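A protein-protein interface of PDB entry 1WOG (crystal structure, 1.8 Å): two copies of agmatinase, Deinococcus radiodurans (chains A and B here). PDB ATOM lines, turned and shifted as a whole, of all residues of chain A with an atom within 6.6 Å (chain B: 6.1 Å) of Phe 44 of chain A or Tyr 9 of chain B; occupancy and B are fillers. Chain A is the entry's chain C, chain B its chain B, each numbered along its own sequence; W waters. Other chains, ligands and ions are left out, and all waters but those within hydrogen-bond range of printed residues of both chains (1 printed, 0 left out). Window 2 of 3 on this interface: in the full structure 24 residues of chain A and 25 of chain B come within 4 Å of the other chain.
Hydrophobic or aromatic side chains of chain B that line the printed part of chain A: Leu 7, Pro 8, Tyr 9 and Leu 287.
Among the printed residues, 9 pairs touch across the chains.
Water W1 lies within hydrogen-bond range of OH of Tyr 9 of chain B and O of Leu 42 of chain A.
Of chain B, only Pro 8, Tyr 9 and Arg 61 come within 4 Å of Phe 44 of chain A.
Of chain A, only Gly 43 and Phe 44 come within 4 Å of Tyr 9 of chain B.
Of the printed residues of chain B, Pro 244 of chain A touches Leu 287.
Of the printed residues of chain A, Pro 8 of chain B touches Gly 43 and Phe 44.
Printed residues of chain A within 4 Å of Leu 287 of chain B: Arg 45 and Pro 244.
Printed residues of chain B within 4 Å of Arg 45 of chain A: Leu 287 (3.8 Å).
Leu 60 of chain B touches none of the printed residues of chain A.
Ala 41 of chain A touches none of the printed residues of chain B.
The nearest residue of chain B that does not touch Phe 44 of chain A is Leu 287 of chain B (4.1 Å).
The nearest printed residue of chain B that does not touch Gly 43 of chain A is Arg 61 of chain B (5.1 Å).
No position is printed for both chains.
Of the 9 pairs that touch across the chains among the printed residues, none has its exchanged pair printed and touching as well.
O of Leu 7 of chain B lies within hydrogen-bond range of NH2 of Arg 17 of chain B (3.3 Å).
NH2 of Arg 45 of chain A lies within hydrogen-bond range of O of Thr 241 of chain A.
N of Arg 45 of chain A sits at hydrogen-bond distance from OG of Ser 242 of chain A, at 3.0 Å.
OG of Ser 243 of chain A lies close to OG of Ser 242 of chain A, at 3.4 Å.
The guanidinium group (NH1) of Arg 61 of chain B is in hydrogen-bond range of the side-chain hydroxyl (OG) of Ser 243 of chain A.
O of Gly 43 of chain A touches CD1 of Leu 7 of chain B (3.7 Å).
Gly 43 of chain A touches Pro 8 of chain B.
Gly 43 of chain A touches Tyr 9 of chain B (O to CE1, 3.3 Å).
Phe 44 of chain A touches Pro 8 of chain B.
O of Phe 44 of chain A touches CD1 of Tyr 9 of chain B, 3.5 Å away.
Arg 61 of chain B touches Phe 44 of chain A.
Arg 45 of chain A touches Leu 287 of chain B (NH2 to CD1, 3.8 Å).
CG of Pro 244 of chain A touches CD1 of Leu 287 of chain B, 3.7 Å away.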
ATOM      1  N   ALA A  41       8.613  -8.775 -24.773  1.00  0.00           N
ATOM      2  CA  ALA A  41      10.073  -8.771 -24.799  1.00  0.00           C
ATOM      3  C   ALA A  41      10.686  -8.695 -23.403  1.00  0.00           C
ATOM      4  O   ALA A  41      11.882  -8.937 -23.240  1.00  0.00           O
ATOM      5  CB  ALA A  41      10.584  -7.619 -25.654  1.00  0.00           C
ATOM      6  N   LEU A  42       9.887  -8.365 -22.390  1.00  0.00           N
ATOM      7  CA  LEU A  42      10.452  -8.280 -21.044  1.00  0.00           C
ATOM      8  C   LEU A  42      10.729  -9.670 -20.469  1.00  0.00           C
ATOM      9  O   LEU A  42      10.092 -10.652 -20.847  1.00  0.00           O
ATOM     10  CB  LEU A  42       9.539  -7.457 -20.120  1.00  0.00           C
ATOM     11  CG  LEU A  42       8.071  -7.811 -19.901  1.00  0.00           C
ATOM     12  CD1 LEU A  42       7.931  -8.980 -18.935  1.00  0.00           C
ATOM     13  CD2 LEU A  42       7.373  -6.578 -19.327  1.00  0.00           C
ATOM     14  N   GLY A  43      11.686  -9.752 -19.555  1.00  0.00           N
ATOM     15  CA  GLY A  43      12.039 -11.047 -19.004  1.00  0.00           C
ATOM     16  C   GLY A  43      11.509 -11.418 -17.636  1.00  0.00           C
ATOM     17  O   GLY A  43      12.030 -12.342 -17.014  1.00  0.00           O
ATOM     18  N   PHE A  44      10.478 -10.729 -17.158  1.00  0.00           N
ATOM     19  CA  PHE A  44       9.950 -11.059 -15.842  1.00  0.00           C
ATOM     20  C   PHE A  44       8.422 -11.003 -15.751  1.00  0.00           C
ATOM     21  O   PHE A  44       7.738 -11.930 -16.180  1.00  0.00           O
ATOM     22  CB  PHE A  44      10.575 -10.134 -14.784  1.00  0.00           C
ATOM     23  CG  PHE A  44      10.306 -10.554 -13.365  1.00  0.00           C
ATOM     24  CD1 PHE A  44      10.417  -9.630 -12.325  1.00  0.00           C
ATOM     25  CD2 PHE A  44       9.959 -11.868 -13.059  1.00  0.00           C
ATOM     26  CE1 PHE A  44      10.188 -10.009 -11.006  1.00  0.00           C
ATOM     27  CE2 PHE A  44       9.728 -12.256 -11.740  1.00  0.00           C
ATOM     28  CZ  PHE A  44       9.843 -11.323 -10.713  1.00  0.00           C
ATOM     29  N   ARG A  45       7.891  -9.914 -15.199  1.00  0.00           N
ATOM     30  CA  ARG A  45       6.446  -9.779 -15.018  1.00  0.00           C
ATOM     31  C   ARG A  45       5.729  -8.966 -16.100  1.00  0.00           C
ATOM     32  O   ARG A  45       5.950  -7.765 -16.246  1.00  0.00           O
ATOM     33  CB  ARG A  45       6.166  -9.177 -13.634  1.00  0.00           C
ATOM     34  CG  ARG A  45       6.799  -9.973 -12.493  1.00  0.00           C
ATOM     35  CD  ARG A  45       6.434  -9.412 -11.122  1.00  0.00           C
ATOM     36  NE  ARG A  45       7.018  -8.092 -10.895  1.00  0.00           N
ATOM     37  CZ  ARG A  45       6.804  -7.358  -9.810  1.00  0.00           C
ATOM     38  NH1 ARG A  45       6.016  -7.816  -8.846  1.00  0.00           N
ATOM     39  NH2 ARG A  45       7.369  -6.162  -9.694  1.00  0.00           N
ATOM     40  N   PRO A  46       4.840  -9.621 -16.864  1.00  0.00           N
ATOM     41  CA  PRO A  46       4.072  -8.989 -17.942  1.00  0.00           C
ATOM     42  C   PRO A  46       3.037  -8.013 -17.383  1.00  0.00           C
ATOM     43  O   PRO A  46       2.736  -8.038 -16.188  1.00  0.00           O
ATOM     44  CB  PRO A  46       3.382 -10.173 -18.632  1.00  0.00           C
ATOM     45  CG  PRO A  46       4.117 -11.382 -18.142  1.00  0.00           C
ATOM     46  CD  PRO A  46       4.470 -11.039 -16.733  1.00  0.00           C
ATOM     47  N   ARG A 152      20.557 -11.268 -25.047  1.00  0.00           N
ATOM     48  CA  ARG A 152      20.095 -11.728 -23.743  1.00  0.00           C
ATOM     49  C   ARG A 152      19.104 -12.857 -23.992  1.00  0.00           C
ATOM     50  O   ARG A 152      18.226 -12.737 -24.844  1.00  0.00           O
ATOM     51  CB  ARG A 152      19.393 -10.595 -22.987  1.00  0.00           C
ATOM     52  CG  ARG A 152      19.079 -10.911 -21.531  1.00  0.00           C
ATOM     53  CD  ARG A 152      17.941 -10.043 -21.011  1.00  0.00           C
ATOM     54  NE  ARG A 152      16.650 -10.513 -21.508  1.00  0.00           N
ATOM     55  CZ  ARG A 152      15.504  -9.863 -21.351  1.00  0.00           C
ATOM     56  NH1 ARG A 152      14.379 -10.372 -21.837  1.00  0.00           N
ATOM     57  NH2 ARG A 152      15.482  -8.698 -20.717  1.00  0.00           N
ATOM     58  N   ASN A 159      13.975  -6.294 -23.933  1.00  0.00           N
ATOM     59  CA  ASN A 159      13.900  -4.930 -23.432  1.00  0.00           C
ATOM     60  C   ASN A 159      15.234  -4.475 -22.832  1.00  0.00           C
ATOM     61  O   ASN A 159      15.352  -3.357 -22.333  1.00  0.00           O
ATOM     62  CB  ASN A 159      12.764  -4.771 -22.405  1.00  0.00           C
ATOM     63  CG  ASN A 159      12.937  -5.643 -21.173  1.00  0.00           C
ATOM     64  OD1 ASN A 159      13.639  -6.655 -21.221  1.00  0.00           O
ATOM     65  ND2 ASN A 159      12.321  -5.253 -20.067  1.00  0.00           N
ATOM     66  N   THR A 241       5.744  -1.906 -11.866  1.00  0.00           N
ATOM     67  CA  THR A 241       6.719  -2.148 -12.923  1.00  0.00           C
ATOM     68  C   THR A 241       7.299  -3.549 -12.739  1.00  0.00           C
ATOM     69  O   THR A 241       7.369  -4.065 -11.623  1.00  0.00           O
ATOM     70  CB  THR A 241       7.833  -1.066 -12.911  1.00  0.00           C
ATOM     71  OG1 THR A 241       8.555  -1.108 -14.150  1.00  0.00           O
ATOM     72  CG2 THR A 241       8.800  -1.291 -11.752  1.00  0.00           C
ATOM     73  N   SER A 242       7.700  -4.171 -13.840  1.00  0.00           N
ATOM     74  CA  SER A 242       8.218  -5.532 -13.796  1.00  0.00           C
ATOM     75  C   SER A 242       9.420  -5.790 -12.900  1.00  0.00           C
ATOM     76  O   SER A 242       9.392  -6.704 -12.067  1.00  0.00           O
ATOM     77  CB  SER A 242       8.557  -6.010 -15.210  1.00  0.00           C
ATOM     78  OG  SER A 242       9.214  -7.272 -15.167  1.00  0.00           O
ATOM     79  N   SER A 243      10.467  -4.988 -13.062  1.00  0.00           N
ATOM     80  CA  SER A 243      11.704  -5.191 -12.309  1.00  0.00           C
ATOM     81  C   SER A 243      12.147  -4.000 -11.472  1.00  0.00           C
ATOM     82  O   SER A 243      13.047  -3.261 -11.863  1.00  0.00           O
ATOM     83  CB  SER A 243      12.821  -5.562 -13.284  1.00  0.00           C
ATOM     84  OG  SER A 243      12.404  -6.609 -14.143  1.00  0.00           O
ATOM     85  N   PRO A 244      11.533  -3.812 -10.295  1.00  0.00           N
ATOM     86  CA  PRO A 244      11.874  -2.701  -9.407  1.00  0.00           C
ATOM     87  C   PRO A 244      13.243  -2.846  -8.744  1.00  0.00           C
ATOM     88  O   PRO A 244      13.714  -3.959  -8.495  1.00  0.00           O
ATOM     89  CB  PRO A 244      10.739  -2.720  -8.388  1.00  0.00           C
ATOM     90  CG  PRO A 244      10.441  -4.188  -8.272  1.00  0.00           C
ATOM     91  CD  PRO A 244      10.455  -4.637  -9.718  1.00  0.00           C
ATOM     92  N   HIS B   6      17.624 -19.968 -17.109  1.00  0.00           N
ATOM     93  CA  HIS B   6      16.213 -19.673 -16.889  1.00  0.00           C
ATOM     94  C   HIS B   6      15.997 -18.200 -16.578  1.00  0.00           C
ATOM     95  O   HIS B   6      16.870 -17.542 -16.010  1.00  0.00           O
ATOM     96  CB  HIS B   6      15.667 -20.472 -15.699  1.00  0.00           C
ATOM     97  CG  HIS B   6      15.220 -21.859 -16.039  1.00  0.00           C
ATOM     98  ND1 HIS B   6      14.261 -22.117 -16.996  1.00  0.00           N
ATOM     99  CD2 HIS B   6      15.564 -23.060 -15.518  1.00  0.00           C
ATOM    100  CE1 HIS B   6      14.033 -23.417 -17.045  1.00  0.00           C
ATOM    101  NE2 HIS B   6      14.811 -24.012 -16.159  1.00  0.00           N
ATOM    102  N   LEU B   7      14.832 -17.687 -16.963  1.00  0.00           N
ATOM    103  CA  LEU B   7      14.463 -16.316 -16.647  1.00  0.00           C
ATOM    104  C   LEU B   7      13.890 -16.472 -15.240  1.00  0.00           C
ATOM    105  O   LEU B   7      13.635 -17.598 -14.799  1.00  0.00           O
ATOM    106  CB  LEU B   7      13.386 -15.795 -17.606  1.00  0.00           C
ATOM    107  CG  LEU B   7      13.804 -15.253 -18.980  1.00  0.00           C
ATOM    108  CD1 LEU B   7      14.754 -14.079 -18.798  1.00  0.00           C
ATOM    109  CD2 LEU B   7      14.460 -16.347 -19.797  1.00  0.00           C
ATOM    110  N   PRO B   8      13.681 -15.362 -14.516  1.00  0.00           N
ATOM    111  CA  PRO B   8      13.139 -15.420 -13.154  1.00  0.00           C
ATOM    112  C   PRO B   8      11.895 -16.288 -12.949  1.00  0.00           C
ATOM    113  O   PRO B   8      11.747 -16.912 -11.899  1.00  0.00           O
ATOM    114  CB  PRO B   8      12.888 -13.951 -12.828  1.00  0.00           C
ATOM    115  CG  PRO B   8      14.026 -13.279 -13.527  1.00  0.00           C
ATOM    116  CD  PRO B   8      14.026 -13.975 -14.877  1.00  0.00           C
ATOM    117  N   TYR B   9      11.006 -16.334 -13.938  1.00  0.00           N
ATOM    118  CA  TYR B   9       9.788 -17.136 -13.803  1.00  0.00           C
ATOM    119  C   TYR B   9       9.967 -18.609 -14.158  1.00  0.00           C
ATOM    120  O   TYR B   9       9.012 -19.384 -14.112  1.00  0.00           O
ATOM    121  CB  TYR B   9       8.658 -16.554 -14.658  1.00  0.00           C
ATOM    122  CG  TYR B   9       9.044 -16.236 -16.083  1.00  0.00           C
ATOM    123  CD1 TYR B   9       9.503 -14.966 -16.431  1.00  0.00           C
ATOM    124  CD2 TYR B   9       8.935 -17.195 -17.090  1.00  0.00           C
ATOM    125  CE1 TYR B   9       9.838 -14.652 -17.745  1.00  0.00           C
ATOM    126  CE2 TYR B   9       9.271 -16.891 -18.416  1.00  0.00           C
ATOM    127  CZ  TYR B   9       9.721 -15.617 -18.732  1.00  0.00           C
ATOM    128  OH  TYR B   9      10.050 -15.297 -20.032  1.00  0.00           O
ATOM    129  N   GLY B  10      11.186 -19.000 -14.510  1.00  0.00           N
ATOM    130  CA  GLY B  10      11.419 -20.388 -14.861  1.00  0.00           C
ATOM    131  C   GLY B  10      12.231 -21.156 -13.835  1.00  0.00           C
ATOM    132  O   GLY B  10      13.031 -20.578 -13.099  1.00  0.00           O
ATOM    133  N   GLY B  11      12.011 -22.467 -13.782  1.00  0.00           N
ATOM    134  CA  GLY B  11      12.748 -23.315 -12.865  1.00  0.00           C
ATOM    135  C   GLY B  11      12.181 -23.455 -11.469  1.00  0.00           C
ATOM    136  O   GLY B  11      11.275 -22.720 -11.066  1.00  0.00           O
ATOM    137  N   ARG B  17      18.892 -19.951  -6.575  1.00  0.00           N
ATOM    138  CA  ARG B  17      18.900 -21.020  -7.565  1.00  0.00           C
ATOM    139  C   ARG B  17      20.001 -22.037  -7.248  1.00  0.00           C
ATOM    140  O   ARG B  17      20.569 -22.658  -8.145  1.00  0.00           O
ATOM    141  CB  ARG B  17      19.087 -20.432  -8.974  1.00  0.00           C
ATOM    142  CG  ARG B  17      18.364 -21.209 -10.074  1.00  0.00           C
ATOM    143  CD  ARG B  17      18.597 -20.612 -11.465  1.00  0.00           C
ATOM    144  NE  ARG B  17      17.656 -19.552 -11.842  1.00  0.00           N
ATOM    145  CZ  ARG B  17      16.353 -19.737 -12.053  1.00  0.00           C
ATOM    146  NH1 ARG B  17      15.816 -20.943 -11.916  1.00  0.00           N
ATOM    147  NH2 ARG B  17      15.589 -18.722 -12.441  1.00  0.00           N
ATOM    148  N   GLU B  57      11.685 -17.427  -4.429  1.00  0.00           N
ATOM    149  CA  GLU B  57      11.233 -17.000  -5.750  1.00  0.00           C
ATOM    150  C   GLU B  57      11.852 -15.656  -6.124  1.00  0.00           C
ATOM    151  O   GLU B  57      12.373 -15.489  -7.225  1.00  0.00           O
ATOM    152  CB  GLU B  57       9.705 -16.892  -5.773  1.00  0.00           C
ATOM    153  CG  GLU B  57       8.992 -18.218  -5.558  1.00  0.00           C
ATOM    154  CD  GLU B  57       7.506 -18.050  -5.301  1.00  0.00           C
ATOM    155  OE1 GLU B  57       6.812 -19.074  -5.139  1.00  0.00           O
ATOM    156  OE2 GLU B  57       7.029 -16.898  -5.259  1.00  0.00           O
ATOM    157  N   LEU B  60      15.474 -15.393  -7.364  1.00  0.00           N
ATOM    158  CA  LEU B  60      15.798 -15.788  -8.732  1.00  0.00           C
ATOM    159  C   LEU B  60      16.172 -14.554  -9.546  1.00  0.00           C
ATOM    160  O   LEU B  60      16.729 -14.660 -10.636  1.00  0.00           O
ATOM    161  CB  LEU B  60      14.623 -16.539  -9.372  1.00  0.00           C
ATOM    162  CG  LEU B  60      14.254 -17.850  -8.661  1.00  0.00           C
ATOM    163  CD1 LEU B  60      13.198 -18.596  -9.467  1.00  0.00           C
ATOM    164  CD2 LEU B  60      15.497 -18.726  -8.487  1.00  0.00           C
ATOM    165  N   ARG B  61      15.863 -13.380  -9.006  1.00  0.00           N
ATOM    166  CA  ARG B  61      16.210 -12.119  -9.655  1.00  0.00           C
ATOM    167  C   ARG B  61      17.610 -11.725  -9.179  1.00  0.00           C
ATOM    168  O   ARG B  61      18.227 -10.812  -9.728  1.00  0.00           O
ATOM    169  CB  ARG B  61      15.224 -11.015  -9.262  1.00  0.00           C
ATOM    170  CG  ARG B  61      13.831 -11.156  -9.839  1.00  0.00           C
ATOM    171  CD  ARG B  61      13.602 -10.158 -10.960  1.00  0.00           C
ATOM    172  NE  ARG B  61      14.562 -10.322 -12.046  1.00  0.00           N
ATOM    173  CZ  ARG B  61      14.516  -9.653 -13.193  1.00  0.00           C
ATOM    174  NH1 ARG B  61      13.554  -8.769 -13.406  1.00  0.00           N
ATOM    175  NH2 ARG B  61      15.429  -9.868 -14.128  1.00  0.00           N
ATOM    176  N   LEU B 287      10.941  -8.928  -3.310  1.00  0.00           N
ATOM    177  CA  LEU B 287      12.008  -8.674  -4.272  1.00  0.00           C
ATOM    178  C   LEU B 287      13.165  -7.907  -3.635  1.00  0.00           C
ATOM    179  O   LEU B 287      14.335  -8.269  -3.803  1.00  0.00           O
ATOM    180  CB  LEU B 287      11.472  -7.897  -5.482  1.00  0.00           C
ATOM    181  CG  LEU B 287      10.579  -8.695  -6.441  1.00  0.00           C
ATOM    182  CD1 LEU B 287      10.038  -7.783  -7.527  1.00  0.00           C
ATOM    183  CD2 LEU B 287      11.383  -9.828  -7.063  1.00  0.00           C
HETATM  184  O   HOH W   1      10.897 -13.285 -21.802  1.00  0.00           O
